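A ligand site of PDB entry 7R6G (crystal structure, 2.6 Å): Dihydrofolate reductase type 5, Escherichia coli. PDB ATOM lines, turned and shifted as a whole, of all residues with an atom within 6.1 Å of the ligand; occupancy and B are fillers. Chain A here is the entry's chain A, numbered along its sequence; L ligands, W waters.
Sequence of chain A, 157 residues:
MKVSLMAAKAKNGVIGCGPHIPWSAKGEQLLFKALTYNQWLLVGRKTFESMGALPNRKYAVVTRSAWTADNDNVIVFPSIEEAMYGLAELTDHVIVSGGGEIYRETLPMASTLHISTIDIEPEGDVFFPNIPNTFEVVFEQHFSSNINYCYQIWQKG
N2 of the ligand is in hydrogen-bond range of OE1 of Glu 105 (2.6 Å).
N of Thr 47 lies close to O1 of the ligand.
The side-chain hydroxyl of Thr 47 sits at hydrogen-bond distance from an oxygen (O1) of the ligand (2.6 Å).
N of Thr 63 lies close to N5 of the ligand.
An oxygen (O16) of the ligand sits at hydrogen-bond distance from the side-chain hydroxyl of Thr 63 (2.6 Å).
The backbone NH of Arg 45 is in hydrogen-bond range of an oxygen (O4) of the ligand, at 3.3 Å.
NH1 of Arg 45 lies within salt-bridge range of O14 of the ligand (2.6 Å).
An oxygen (O1) of the ligand sits close to the backbone NH (N) of Gly 99, 3.3 Å away.
The backbone NH (N) of Arg 64 sits at hydrogen-bond distance from an oxygen (O15) of the ligand, 2.9 Å away.
O8 of the ligand is in hydrogen-bond range of N of Glu 101 (3.0 Å).
SG of Cys 17 is in hydrogen-bond range of N6 of the ligand, 3.0 Å away.
N of Gly 100 lies within hydrogen-bond range of O9 of the ligand.
The side-chain hydroxyl of Ser 65 sits at hydrogen-bond distance from an oxygen (O16) of the ligand (3.3 Å).
O2 of the ligand sits close to N of Ile 102, at 3.5 Å.
An oxygen (O3) of the ligand is in hydrogen-bond range of the backbone NH (N) of Lys 46, at 3.4 Å.
The guanidinium group of Arg 64 is in salt-bridge range of the side-chain carboxylate of Glu 105.
N of Gly 99 is in hydrogen-bond range of OG1 of Thr 47, at 3.1 Å.
The side-chain hydroxyl (OG) of Ser 50 is in hydrogen-bond range of the backbone carbonyl oxygen (O) of Thr 47 (3.1 Å).
The backbone NH (N) of Ser 65 is in hydrogen-bond range of the side-chain hydroxyl (OG1) of Thr 63, at 3.1 Å.
The backbone carbonyl oxygen of Phe 77 is in hydrogen-bond range of the backbone NH of Thr 63 (3.2 Å).
The guanidinium group (NH1) of Arg 64 lies within salt-bridge range of the side-chain carboxylate (OE2) of Glu 101 (3.0 Å).
The backbone NH of Gly 44 lies within hydrogen-bond range of the backbone carbonyl oxygen of Gly 98, at 3.0 Å.
The backbone NH (N) of Asp 125 lies within hydrogen-bond range of the backbone carbonyl oxygen (O) of Gly 16, at 3.4 Å.
Merely in contact with the ligand: Gly 18 (3.7 Å), Gly 44 (3.5 Å), Val 62 (3.2 Å), Pro 78 (3.3 Å), Ser 79 (3.6 Å), Ile 80 (3.7 Å), Gly 98 (3.9 Å), Gly 124 (3.9 Å), Asp 125 (3.9 Å) and Val 126 (3.9 Å).
Hydrophobic or aromatic side chains that line the ligand: Val 62, Ile 80, Ile 102 and Val 126.
Within 4 Å of the ligand: Cys 17, Gly 18, Gly 44, Arg 45, Lys 46, Thr 47, Val 62, Thr 63, Arg 64, Ser 65, Pro 78, Ser 79, Ile 80, Gly 98, Gly 99, Gly 100, Glu 101, Ile 102, Glu 105, Gly 124, Asp 125 and Val 126.
Water W1 bridges N4 of the ligand (2.8 Å) and O of Pro 78 (3.0 Å).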
ATOM      1  N   ILE A  15     -30.562 -11.000   1.539  1.00  0.00           N
ATOM      2  CA  ILE A  15     -30.068  -9.634   1.846  1.00  0.00           C
ATOM      3  C   ILE A  15     -28.553  -9.538   1.714  1.00  0.00           C
ATOM      4  O   ILE A  15     -28.041  -8.447   1.911  1.00  0.00           O
ATOM      5  CB  ILE A  15     -30.477  -9.124   3.238  1.00  0.00           C
ATOM      6  CG1 ILE A  15     -29.800  -9.901   4.350  1.00  0.00           C
ATOM      7  CG2 ILE A  15     -31.982  -9.070   3.411  1.00  0.00           C
ATOM      8  CD1 ILE A  15     -30.284  -9.480   5.690  1.00  0.00           C
ATOM      9  N   GLY A  16     -27.840 -10.612   1.442  1.00  0.00           N
ATOM     10  CA  GLY A  16     -26.362 -10.570   1.453  1.00  0.00           C
ATOM     11  C   GLY A  16     -25.770 -11.831   0.874  1.00  0.00           C
ATOM     12  O   GLY A  16     -26.267 -12.904   1.183  1.00  0.00           O
ATOM     13  N   CYS A  17     -24.750 -11.663   0.024  1.00  0.00           N
ATOM     14  CA  CYS A  17     -23.800 -12.700  -0.440  1.00  0.00           C
ATOM     15  C   CYS A  17     -22.423 -12.290   0.111  1.00  0.00           C
ATOM     16  O   CYS A  17     -21.805 -11.398  -0.521  1.00  0.00           O
ATOM     17  CB  CYS A  17     -23.787 -12.805  -1.964  1.00  0.00           C
ATOM     18  SG  CYS A  17     -22.375 -13.744  -2.590  1.00  0.00           S
ATOM     19  N   GLY A  18     -22.044 -12.850   1.268  1.00  0.00           N
ATOM     20  CA  GLY A  18     -20.917 -12.326   2.085  1.00  0.00           C
ATOM     21  C   GLY A  18     -21.114 -10.845   2.384  1.00  0.00           C
ATOM     22  O   GLY A  18     -22.235 -10.420   2.710  1.00  0.00           O
ATOM     23  N   PRO A  19     -20.062 -10.003   2.265  1.00  0.00           N
ATOM     24  CA  PRO A  19     -20.170  -8.565   2.585  1.00  0.00           C
ATOM     25  C   PRO A  19     -20.709  -7.681   1.448  1.00  0.00           C
ATOM     26  O   PRO A  19     -20.537  -6.488   1.554  1.00  0.00           O
ATOM     27  CB  PRO A  19     -18.708  -8.184   2.898  1.00  0.00           C
ATOM     28  CG  PRO A  19     -17.897  -9.074   1.984  1.00  0.00           C
ATOM     29  CD  PRO A  19     -18.691 -10.360   1.852  1.00  0.00           C
ATOM     30  N   VAL A  43     -26.879  -0.879  13.930  1.00  0.00           N
ATOM     31  CA  VAL A  43     -26.261  -1.817  12.949  1.00  0.00           C
ATOM     32  C   VAL A  43     -25.319  -2.762  13.714  1.00  0.00           C
ATOM     33  O   VAL A  43     -24.651  -2.322  14.663  1.00  0.00           O
ATOM     34  CB  VAL A  43     -25.478  -1.082  11.873  1.00  0.00           C
ATOM     35  CG1 VAL A  43     -26.373  -0.436  10.850  1.00  0.00           C
ATOM     36  CG2 VAL A  43     -24.618  -0.048  12.512  1.00  0.00           C
ATOM     37  N   GLY A  44     -25.291  -4.021  13.299  1.00  0.00           N
ATOM     38  CA  GLY A  44     -24.239  -4.965  13.693  1.00  0.00           C
ATOM     39  C   GLY A  44     -22.898  -4.534  13.144  1.00  0.00           C
ATOM     40  O   GLY A  44     -22.839  -3.755  12.152  1.00  0.00           O
ATOM     41  N   ARG A  45     -21.843  -5.011  13.792  1.00  0.00           N
ATOM     42  CA  ARG A  45     -20.475  -4.565  13.511  1.00  0.00           C
ATOM     43  C   ARG A  45     -20.086  -4.983  12.073  1.00  0.00           C
ATOM     44  O   ARG A  45     -19.298  -4.233  11.484  1.00  0.00           O
ATOM     45  CB  ARG A  45     -19.538  -5.144  14.569  1.00  0.00           C
ATOM     46  CG  ARG A  45     -18.093  -4.679  14.454  1.00  0.00           C
ATOM     47  CD  ARG A  45     -17.186  -5.503  13.573  1.00  0.00           C
ATOM     48  NE  ARG A  45     -17.239  -6.902  13.899  1.00  0.00           N
ATOM     49  CZ  ARG A  45     -16.935  -7.860  13.053  1.00  0.00           C
ATOM     50  NH1 ARG A  45     -17.073  -9.101  13.421  1.00  0.00           N
ATOM     51  NH2 ARG A  45     -16.530  -7.568  11.830  1.00  0.00           N
ATOM     52  N   LYS A  46     -20.576  -6.121  11.556  1.00  0.00           N
ATOM     53  CA  LYS A  46     -20.146  -6.637  10.226  1.00  0.00           C
ATOM     54  C   LYS A  46     -20.712  -5.705   9.172  1.00  0.00           C
ATOM     55  O   LYS A  46     -19.936  -5.283   8.278  1.00  0.00           O
ATOM     56  CB  LYS A  46     -20.568  -8.074   9.956  1.00  0.00           C
ATOM     57  CG  LYS A  46     -19.748  -9.128  10.707  1.00  0.00           C
ATOM     58  CD  LYS A  46     -20.262 -10.530  10.512  1.00  0.00           C
ATOM     59  CE  LYS A  46     -19.638 -11.560  11.426  1.00  0.00           C
ATOM     60  NZ  LYS A  46     -19.975 -12.958  11.027  1.00  0.00           N
ATOM     61  N   THR A  47     -21.985  -5.347   9.317  1.00  0.00           N
ATOM     62  CA  THR A  47     -22.698  -4.496   8.339  1.00  0.00           C
ATOM     63  C   THR A  47     -22.038  -3.126   8.373  1.00  0.00           C
ATOM     64  O   THR A  47     -21.906  -2.497   7.298  1.00  0.00           O
ATOM     65  CB  THR A  47     -24.216  -4.484   8.601  1.00  0.00           C
ATOM     66  OG1 THR A  47     -24.797  -5.688   8.079  1.00  0.00           O
ATOM     67  CG2 THR A  47     -24.931  -3.303   7.982  1.00  0.00           C
ATOM     68  N   PHE A  48     -21.640  -2.674   9.557  1.00  0.00           N
ATOM     69  CA  PHE A  48     -21.100  -1.314   9.719  1.00  0.00           C
ATOM     70  C   PHE A  48     -19.766  -1.215   8.965  1.00  0.00           C
ATOM     71  O   PHE A  48     -19.468  -0.197   8.325  1.00  0.00           O
ATOM     72  CB  PHE A  48     -21.026  -0.917  11.205  1.00  0.00           C
ATOM     73  CG  PHE A  48     -20.528   0.489  11.403  1.00  0.00           C
ATOM     74  CD1 PHE A  48     -21.371   1.564  11.209  1.00  0.00           C
ATOM     75  CD2 PHE A  48     -19.199   0.749  11.655  1.00  0.00           C
ATOM     76  CE1 PHE A  48     -20.909   2.861  11.400  1.00  0.00           C
ATOM     77  CE2 PHE A  48     -18.745   2.043  11.840  1.00  0.00           C
ATOM     78  CZ  PHE A  48     -19.601   3.099  11.706  1.00  0.00           C
ATOM     79  N   SER A  50     -18.704  -3.252   6.461  1.00  0.00           N
ATOM     80  CA  SER A  50     -18.887  -3.510   5.009  1.00  0.00           C
ATOM     81  C   SER A  50     -19.577  -2.307   4.363  1.00  0.00           C
ATOM     82  O   SER A  50     -19.349  -2.107   3.194  1.00  0.00           O
ATOM     83  CB  SER A  50     -19.648  -4.768   4.784  1.00  0.00           C
ATOM     84  OG  SER A  50     -21.000  -4.514   5.080  1.00  0.00           O
ATOM     85  N   VAL A  62     -23.180  -2.598  17.722  1.00  0.00           N
ATOM     86  CA  VAL A  62     -23.003  -3.604  18.809  1.00  0.00           C
ATOM     87  C   VAL A  62     -21.915  -4.582  18.392  1.00  0.00           C
ATOM     88  O   VAL A  62     -21.843  -4.921  17.203  1.00  0.00           O
ATOM     89  CB  VAL A  62     -24.316  -4.323  19.153  1.00  0.00           C
ATOM     90  CG1 VAL A  62     -25.320  -3.378  19.750  1.00  0.00           C
ATOM     91  CG2 VAL A  62     -24.866  -5.022  17.919  1.00  0.00           C
ATOM     92  N   THR A  63     -21.089  -4.982  19.346  1.00  0.00           N
ATOM     93  CA  THR A  63     -20.005  -5.976  19.167  1.00  0.00           C
ATOM     94  C   THR A  63     -19.971  -6.823  20.443  1.00  0.00           C
ATOM     95  O   THR A  63     -20.456  -6.313  21.539  1.00  0.00           O
ATOM     96  CB  THR A  63     -18.675  -5.273  18.841  1.00  0.00           C
ATOM     97  OG1 THR A  63     -17.576  -6.180  18.723  1.00  0.00           O
ATOM     98  CG2 THR A  63     -18.307  -4.235  19.876  1.00  0.00           C
ATOM     99  N   ARG A  64     -19.504  -8.072  20.303  1.00  0.00           N
ATOM    100  CA  ARG A  64     -19.178  -8.952  21.464  1.00  0.00           C
ATOM    101  C   ARG A  64     -17.661  -8.921  21.719  1.00  0.00           C
ATOM    102  O   ARG A  64     -17.269  -9.490  22.758  1.00  0.00           O
ATOM    103  CB  ARG A  64     -19.698 -10.375  21.233  1.00  0.00           C
ATOM    104  CG  ARG A  64     -21.218 -10.437  21.115  1.00  0.00           C
ATOM    105  CD  ARG A  64     -21.748 -11.860  21.174  1.00  0.00           C
ATOM    106  NE  ARG A  64     -23.197 -11.927  21.051  1.00  0.00           N
ATOM    107  CZ  ARG A  64     -23.869 -11.992  19.906  1.00  0.00           C
ATOM    108  NH1 ARG A  64     -23.247 -11.997  18.733  1.00  0.00           N
ATOM    109  NH2 ARG A  64     -25.196 -12.012  19.926  1.00  0.00           N
ATOM    110  N   SER A  65     -16.857  -8.265  20.840  1.00  0.00           N
ATOM    111  CA  SER A  65     -15.389  -8.034  21.038  1.00  0.00           C
ATOM    112  C   SER A  65     -15.186  -6.685  21.742  1.00  0.00           C
ATOM    113  O   SER A  65     -16.182  -6.061  22.209  1.00  0.00           O
ATOM    114  CB  SER A  65     -14.476  -8.010  19.792  1.00  0.00           C
ATOM    115  OG  SER A  65     -15.083  -8.477  18.617  1.00  0.00           O
ATOM    116  N   TRP A  67     -13.915  -4.396  19.795  1.00  0.00           N
ATOM    117  CA  TRP A  67     -13.972  -3.602  18.537  1.00  0.00           C
ATOM    118  C   TRP A  67     -14.407  -2.169  18.864  1.00  0.00           C
ATOM    119  O   TRP A  67     -15.252  -1.987  19.774  1.00  0.00           O
ATOM    120  CB  TRP A  67     -14.937  -4.268  17.548  1.00  0.00           C
ATOM    121  CG  TRP A  67     -14.965  -3.629  16.199  1.00  0.00           C
ATOM    122  CD1 TRP A  67     -14.189  -3.967  15.123  1.00  0.00           C
ATOM    123  CD2 TRP A  67     -15.763  -2.513  15.789  1.00  0.00           C
ATOM    124  NE1 TRP A  67     -14.457  -3.126  14.074  1.00  0.00           N
ATOM    125  CE2 TRP A  67     -15.405  -2.211  14.453  1.00  0.00           C
ATOM    126  CE3 TRP A  67     -16.759  -1.738  16.413  1.00  0.00           C
ATOM    127  CZ2 TRP A  67     -16.021  -1.190  13.738  1.00  0.00           C
ATOM    128  CZ3 TRP A  67     -17.335  -0.692  15.720  1.00  0.00           C
ATOM    129  CH2 TRP A  67     -16.973  -0.432  14.398  1.00  0.00           C
ATOM    130  N   PHE A  77     -21.715  -0.471  21.695  1.00  0.00           N
ATOM    131  CA  PHE A  77     -22.329  -1.074  22.884  1.00  0.00           C
ATOM    132  C   PHE A  77     -21.993  -2.542  22.875  1.00  0.00           C
ATOM    133  O   PHE A  77     -21.781  -3.092  21.800  1.00  0.00           O
ATOM    134  CB  PHE A  77     -23.831  -0.815  22.876  1.00  0.00           C
ATOM    135  CG  PHE A  77     -24.228   0.623  22.996  1.00  0.00           C
ATOM    136  CD1 PHE A  77     -24.419   1.402  21.855  1.00  0.00           C
ATOM    137  CD2 PHE A  77     -24.503   1.193  24.234  1.00  0.00           C
ATOM    138  CE1 PHE A  77     -24.851   2.721  21.953  1.00  0.00           C
ATOM    139  CE2 PHE A  77     -24.934   2.502  24.317  1.00  0.00           C
ATOM    140  CZ  PHE A  77     -25.131   3.258  23.177  1.00  0.00           C
ATOM    141  N   PRO A  78     -21.876  -3.181  24.072  1.00  0.00           N
ATOM    142  CA  PRO A  78     -21.566  -4.612  24.168  1.00  0.00           C
ATOM    143  C   PRO A  78     -22.796  -5.513  23.982  1.00  0.00           C
ATOM    144  O   PRO A  78     -22.628  -6.728  23.880  1.00  0.00           O
ATOM    145  CB  PRO A  78     -21.017  -4.728  25.608  1.00  0.00           C
ATOM    146  CG  PRO A  78     -21.818  -3.687  26.391  1.00  0.00           C
ATOM    147  CD  PRO A  78     -21.977  -2.541  25.408  1.00  0.00           C
ATOM    148  N   SER A  79     -23.997  -4.913  23.940  1.00  0.00           N
ATOM    149  CA  SER A  79     -25.276  -5.620  23.769  1.00  0.00           C
ATOM    150  C   SER A  79     -26.364  -4.691  23.224  1.00  0.00           C
ATOM    151  O   SER A  79     -26.260  -3.471  23.357  1.00  0.00           O
ATOM    152  CB  SER A  79     -25.715  -6.250  25.064  1.00  0.00           C
ATOM    153  OG  SER A  79     -26.101  -5.254  26.003  1.00  0.00           O
ATOM    154  N   ILE A  80     -27.453  -5.284  22.731  1.00  0.00           N
ATOM    155  CA  ILE A  80     -28.619  -4.545  22.201  1.00  0.00           C
ATOM    156  C   ILE A  80     -29.355  -3.910  23.369  1.00  0.00           C
ATOM    157  O   ILE A  80     -29.839  -2.809  23.219  1.00  0.00           O
ATOM    158  CB  ILE A  80     -29.479  -5.480  21.346  1.00  0.00           C
ATOM    159  CG1 ILE A  80     -28.668  -5.914  20.127  1.00  0.00           C
ATOM    160  CG2 ILE A  80     -30.799  -4.842  20.980  1.00  0.00           C
ATOM    161  CD1 ILE A  80     -29.340  -6.938  19.268  1.00  0.00           C
ATOM    162  N   GLY A  98     -29.732  -3.209  10.140  1.00  0.00           N
ATOM    163  CA  GLY A  98     -29.285  -4.509   9.651  1.00  0.00           C
ATOM    164  C   GLY A  98     -27.971  -5.044  10.204  1.00  0.00           C
ATOM    165  O   GLY A  98     -27.378  -4.483  11.165  1.00  0.00           O
ATOM    166  N   GLY A  99     -27.515  -6.045   9.432  1.00  0.00           N
ATOM    167  CA  GLY A  99     -27.233  -7.419   9.834  1.00  0.00           C
ATOM    168  C   GLY A  99     -28.459  -8.310   9.690  1.00  0.00           C
ATOM    169  O   GLY A  99     -29.528  -7.964  10.223  1.00  0.00           O
ATOM    170  N   GLY A 100     -28.290  -9.483   9.085  1.00  0.00           N
ATOM    171  CA  GLY A 100     -29.217 -10.614   9.270  1.00  0.00           C
ATOM    172  C   GLY A 100     -29.367 -10.996  10.742  1.00  0.00           C
ATOM    173  O   GLY A 100     -30.504 -11.079  11.210  1.00  0.00           O
ATOM    174  N   GLU A 101     -28.275 -11.176  11.469  1.00  0.00           N
ATOM    175  CA  GLU A 101     -28.276 -11.469  12.929  1.00  0.00           C
ATOM    176  C   GLU A 101     -29.089 -10.385  13.656  1.00  0.00           C
ATOM    177  O   GLU A 101     -30.048 -10.736  14.366  1.00  0.00           O
ATOM    178  CB  GLU A 101     -26.838 -11.590  13.443  1.00  0.00           C
ATOM    179  CG  GLU A 101     -26.767 -11.964  14.912  1.00  0.00           C
ATOM    180  CD  GLU A 101     -25.411 -12.406  15.435  1.00  0.00           C
ATOM    181  OE1 GLU A 101     -24.480 -12.593  14.603  1.00  0.00           O
ATOM    182  OE2 GLU A 101     -25.297 -12.567  16.665  1.00  0.00           O
ATOM    183  N   ILE A 102     -28.787  -9.112  13.416  1.00  0.00           N
ATOM    184  CA  ILE A 102     -29.437  -7.977  14.128  1.00  0.00           C
ATOM    185  C   ILE A 102     -30.939  -7.970  13.870  1.00  0.00           C
ATOM    186  O   ILE A 102     -31.690  -7.559  14.776  1.00  0.00           O
ATOM    187  CB  ILE A 102     -28.789  -6.645  13.675  1.00  0.00           C
ATOM    188  CG1 ILE A 102     -27.354  -6.564  14.175  1.00  0.00           C
ATOM    189  CG2 ILE A 102     -29.591  -5.446  14.148  1.00  0.00           C
ATOM    190  CD1 ILE A 102     -27.268  -6.548  15.674  1.00  0.00           C
ATOM    191  N   TYR A 103     -31.341  -8.281  12.629  1.00  0.00           N
ATOM    192  CA  TYR A 103     -32.747  -8.215  12.181  1.00  0.00           C
ATOM    193  C   TYR A 103     -33.498  -9.284  12.966  1.00  0.00           C
ATOM    194  O   TYR A 103     -34.589  -8.972  13.560  1.00  0.00           O
ATOM    195  CB  TYR A 103     -32.839  -8.403  10.661  1.00  0.00           C
ATOM    196  CG  TYR A 103     -32.540  -7.198   9.783  1.00  0.00           C
ATOM    197  CD1 TYR A 103     -32.893  -5.908  10.133  1.00  0.00           C
ATOM    198  CD2 TYR A 103     -31.972  -7.379   8.534  1.00  0.00           C
ATOM    199  CE1 TYR A 103     -32.674  -4.842   9.284  1.00  0.00           C
ATOM    200  CE2 TYR A 103     -31.714  -6.319   7.671  1.00  0.00           C
ATOM    201  CZ  TYR A 103     -32.084  -5.057   8.039  1.00  0.00           C
ATOM    202  OH  TYR A 103     -31.876  -4.067   7.135  1.00  0.00           O
ATOM    203  N   GLU A 105     -32.625 -10.596  15.813  1.00  0.00           N
ATOM    204  CA  GLU A 105     -32.583 -10.285  17.276  1.00  0.00           C
ATOM    205  C   GLU A 105     -33.541  -9.172  17.684  1.00  0.00           C
ATOM    206  O   GLU A 105     -33.788  -9.071  18.884  1.00  0.00           O
ATOM    207  CB  GLU A 105     -31.187  -9.849  17.687  1.00  0.00           C
ATOM    208  CG  GLU A 105     -30.206 -11.006  17.613  1.00  0.00           C
ATOM    209  CD  GLU A 105     -28.810 -10.671  18.103  1.00  0.00           C
ATOM    210  OE1 GLU A 105     -27.993 -10.184  17.281  1.00  0.00           O
ATOM    211  OE2 GLU A 105     -28.537 -10.877  19.313  1.00  0.00           O
ATOM    212  N   GLU A 123     -28.192 -15.699  -5.555  1.00  0.00           N
ATOM    213  CA  GLU A 123     -27.530 -16.622  -4.583  1.00  0.00           C
ATOM    214  C   GLU A 123     -27.146 -15.838  -3.320  1.00  0.00           C
ATOM    215  O   GLU A 123     -26.753 -14.645  -3.439  1.00  0.00           O
ATOM    216  CB  GLU A 123     -26.241 -17.237  -5.153  1.00  0.00           C
ATOM    217  CG  GLU A 123     -26.392 -17.940  -6.487  1.00  0.00           C
ATOM    218  CD  GLU A 123     -26.369 -19.455  -6.418  1.00  0.00           C
ATOM    219  OE1 GLU A 123     -25.248 -20.049  -6.427  1.00  0.00           O
ATOM    220  OE2 GLU A 123     -27.474 -20.046  -6.355  1.00  0.00           O
ATOM    221  N   GLY A 124     -27.236 -16.469  -2.144  1.00  0.00           N
ATOM    222  CA  GLY A 124     -27.201 -15.719  -0.883  1.00  0.00           C
ATOM    223  C   GLY A 124     -26.835 -16.513   0.341  1.00  0.00           C
ATOM    224  O   GLY A 124     -27.648 -17.320   0.835  1.00  0.00           O
ATOM    225  N   ASP A 125     -25.666 -16.202   0.887  1.00  0.00           N
ATOM    226  CA  ASP A 125     -25.261 -16.457   2.289  1.00  0.00           C
ATOM    227  C   ASP A 125     -26.375 -16.017   3.288  1.00  0.00           C
ATOM    228  O   ASP A 125     -26.791 -16.854   4.091  1.00  0.00           O
ATOM    229  CB  ASP A 125     -23.895 -15.788   2.394  1.00  0.00           C
ATOM    230  CG  ASP A 125     -23.162 -16.009   3.688  1.00  0.00           C
ATOM    231  OD1 ASP A 125     -23.802 -16.491   4.651  1.00  0.00           O
ATOM    232  OD2 ASP A 125     -21.952 -15.675   3.737  1.00  0.00           O
ATOM    233  N   VAL A 126     -26.899 -14.788   3.238  1.00  0.00           N
ATOM    234  CA  VAL A 126     -27.700 -14.139   4.331  1.00  0.00           C
ATOM    235  C   VAL A 126     -29.149 -13.856   3.897  1.00  0.00           C
ATOM    236  O   VAL A 126     -29.364 -13.501   2.734  1.00  0.00           O
ATOM    237  CB  VAL A 126     -27.034 -12.823   4.759  1.00  0.00           C
ATOM    238  CG1 VAL A 126     -27.478 -12.401   6.149  1.00  0.00           C
ATOM    239  CG2 VAL A 126     -25.514 -12.910   4.684  1.00  0.00           C
HETATM  240  P1  LIG L   1     -24.486  -8.181  11.197  1.00  0.00           P
HETATM  241  O1  LIG L   1     -24.448  -6.978  10.322  1.00  0.00           O
HETATM  242  O2  LIG L   1     -25.721  -8.541  11.935  1.00  0.00           O
HETATM  243  O3  LIG L   1     -23.239  -8.170  12.219  1.00  0.00           O
HETATM  244  C1  LIG L   1     -23.270  -9.146  13.278  1.00  0.00           C
HETATM  245  C2  LIG L   1     -22.275  -8.749  14.327  1.00  0.00           C
HETATM  246  O4  LIG L   1     -22.877  -7.757  15.212  1.00  0.00           O
HETATM  247  C3  LIG L   1     -21.782  -9.863  15.266  1.00  0.00           C
HETATM  248  O5  LIG L   1     -20.786 -10.636  14.605  1.00  0.00           O
HETATM  249  C4  LIG L   1     -21.341  -9.021  16.461  1.00  0.00           C
HETATM  250  O6  LIG L   1     -20.148  -8.203  16.389  1.00  0.00           O
HETATM  251  C5  LIG L   1     -22.474  -7.986  16.535  1.00  0.00           C
HETATM  252  N1  LIG L   1     -23.633  -8.375  17.338  1.00  0.00           N
HETATM  253  C6  LIG L   1     -24.815  -8.921  16.897  1.00  0.00           C
HETATM  254  N2  LIG L   1     -25.692  -9.117  17.844  1.00  0.00           N
HETATM  255  C7  LIG L   1     -25.073  -8.687  19.003  1.00  0.00           C
HETATM  256  C8  LIG L   1     -25.491  -8.649  20.355  1.00  0.00           C
HETATM  257  N3  LIG L   1     -26.685  -9.030  20.806  1.00  0.00           N
HETATM  258  N4  LIG L   1     -24.608  -8.136  21.244  1.00  0.00           N
HETATM  259  C9  LIG L   1     -23.417  -7.724  20.801  1.00  0.00           C
HETATM  260  N5  LIG L   1     -22.928  -7.711  19.572  1.00  0.00           N
HETATM  261  C10 LIG L   1     -23.804  -8.213  18.703  1.00  0.00           C
HETATM  262  O7  LIG L   1     -24.057  -9.432  10.331  1.00  0.00           O
HETATM  263  P2  LIG L   1     -24.766 -10.373   9.277  1.00  0.00           P
HETATM  264  O8  LIG L   1     -25.642 -11.326  10.005  1.00  0.00           O
HETATM  265  O9  LIG L   1     -25.328  -9.615   8.123  1.00  0.00           O
HETATM  266  O10 LIG L   1     -23.459 -11.147   8.805  1.00  0.00           O
HETATM  267  C11 LIG L   1     -23.200 -11.446   7.418  1.00  0.00           C
HETATM  268  C12 LIG L   1     -21.727 -11.784   7.310  1.00  0.00           C
HETATM  269  O11 LIG L   1     -21.530 -13.213   7.211  1.00  0.00           O
HETATM  270  C13 LIG L   1     -20.963 -11.177   6.108  1.00  0.00           C
HETATM  271  O12 LIG L   1     -20.370  -9.926   6.456  1.00  0.00           O
HETATM  272  C14 LIG L   1     -19.996 -12.341   5.728  1.00  0.00           C
HETATM  273  O13 LIG L   1     -18.620 -11.956   5.618  1.00  0.00           O
HETATM  274  C15 LIG L   1     -20.193 -13.423   6.795  1.00  0.00           C
HETATM  275  N6  LIG L   1     -23.346 -16.574  -2.201  1.00  0.00           N
HETATM  276  P3  LIG L   1     -18.696  -8.926  16.667  1.00  0.00           P
HETATM  277  O14 LIG L   1     -18.504  -9.863  15.496  1.00  0.00           O
HETATM  278  O15 LIG L   1     -18.748  -9.661  18.045  1.00  0.00           O
HETATM  279  O16 LIG L   1     -17.684  -7.762  16.632  1.00  0.00           O
HETATM  280  O   HOH W   1     -24.380  -9.212  23.795  1.00  0.00           O
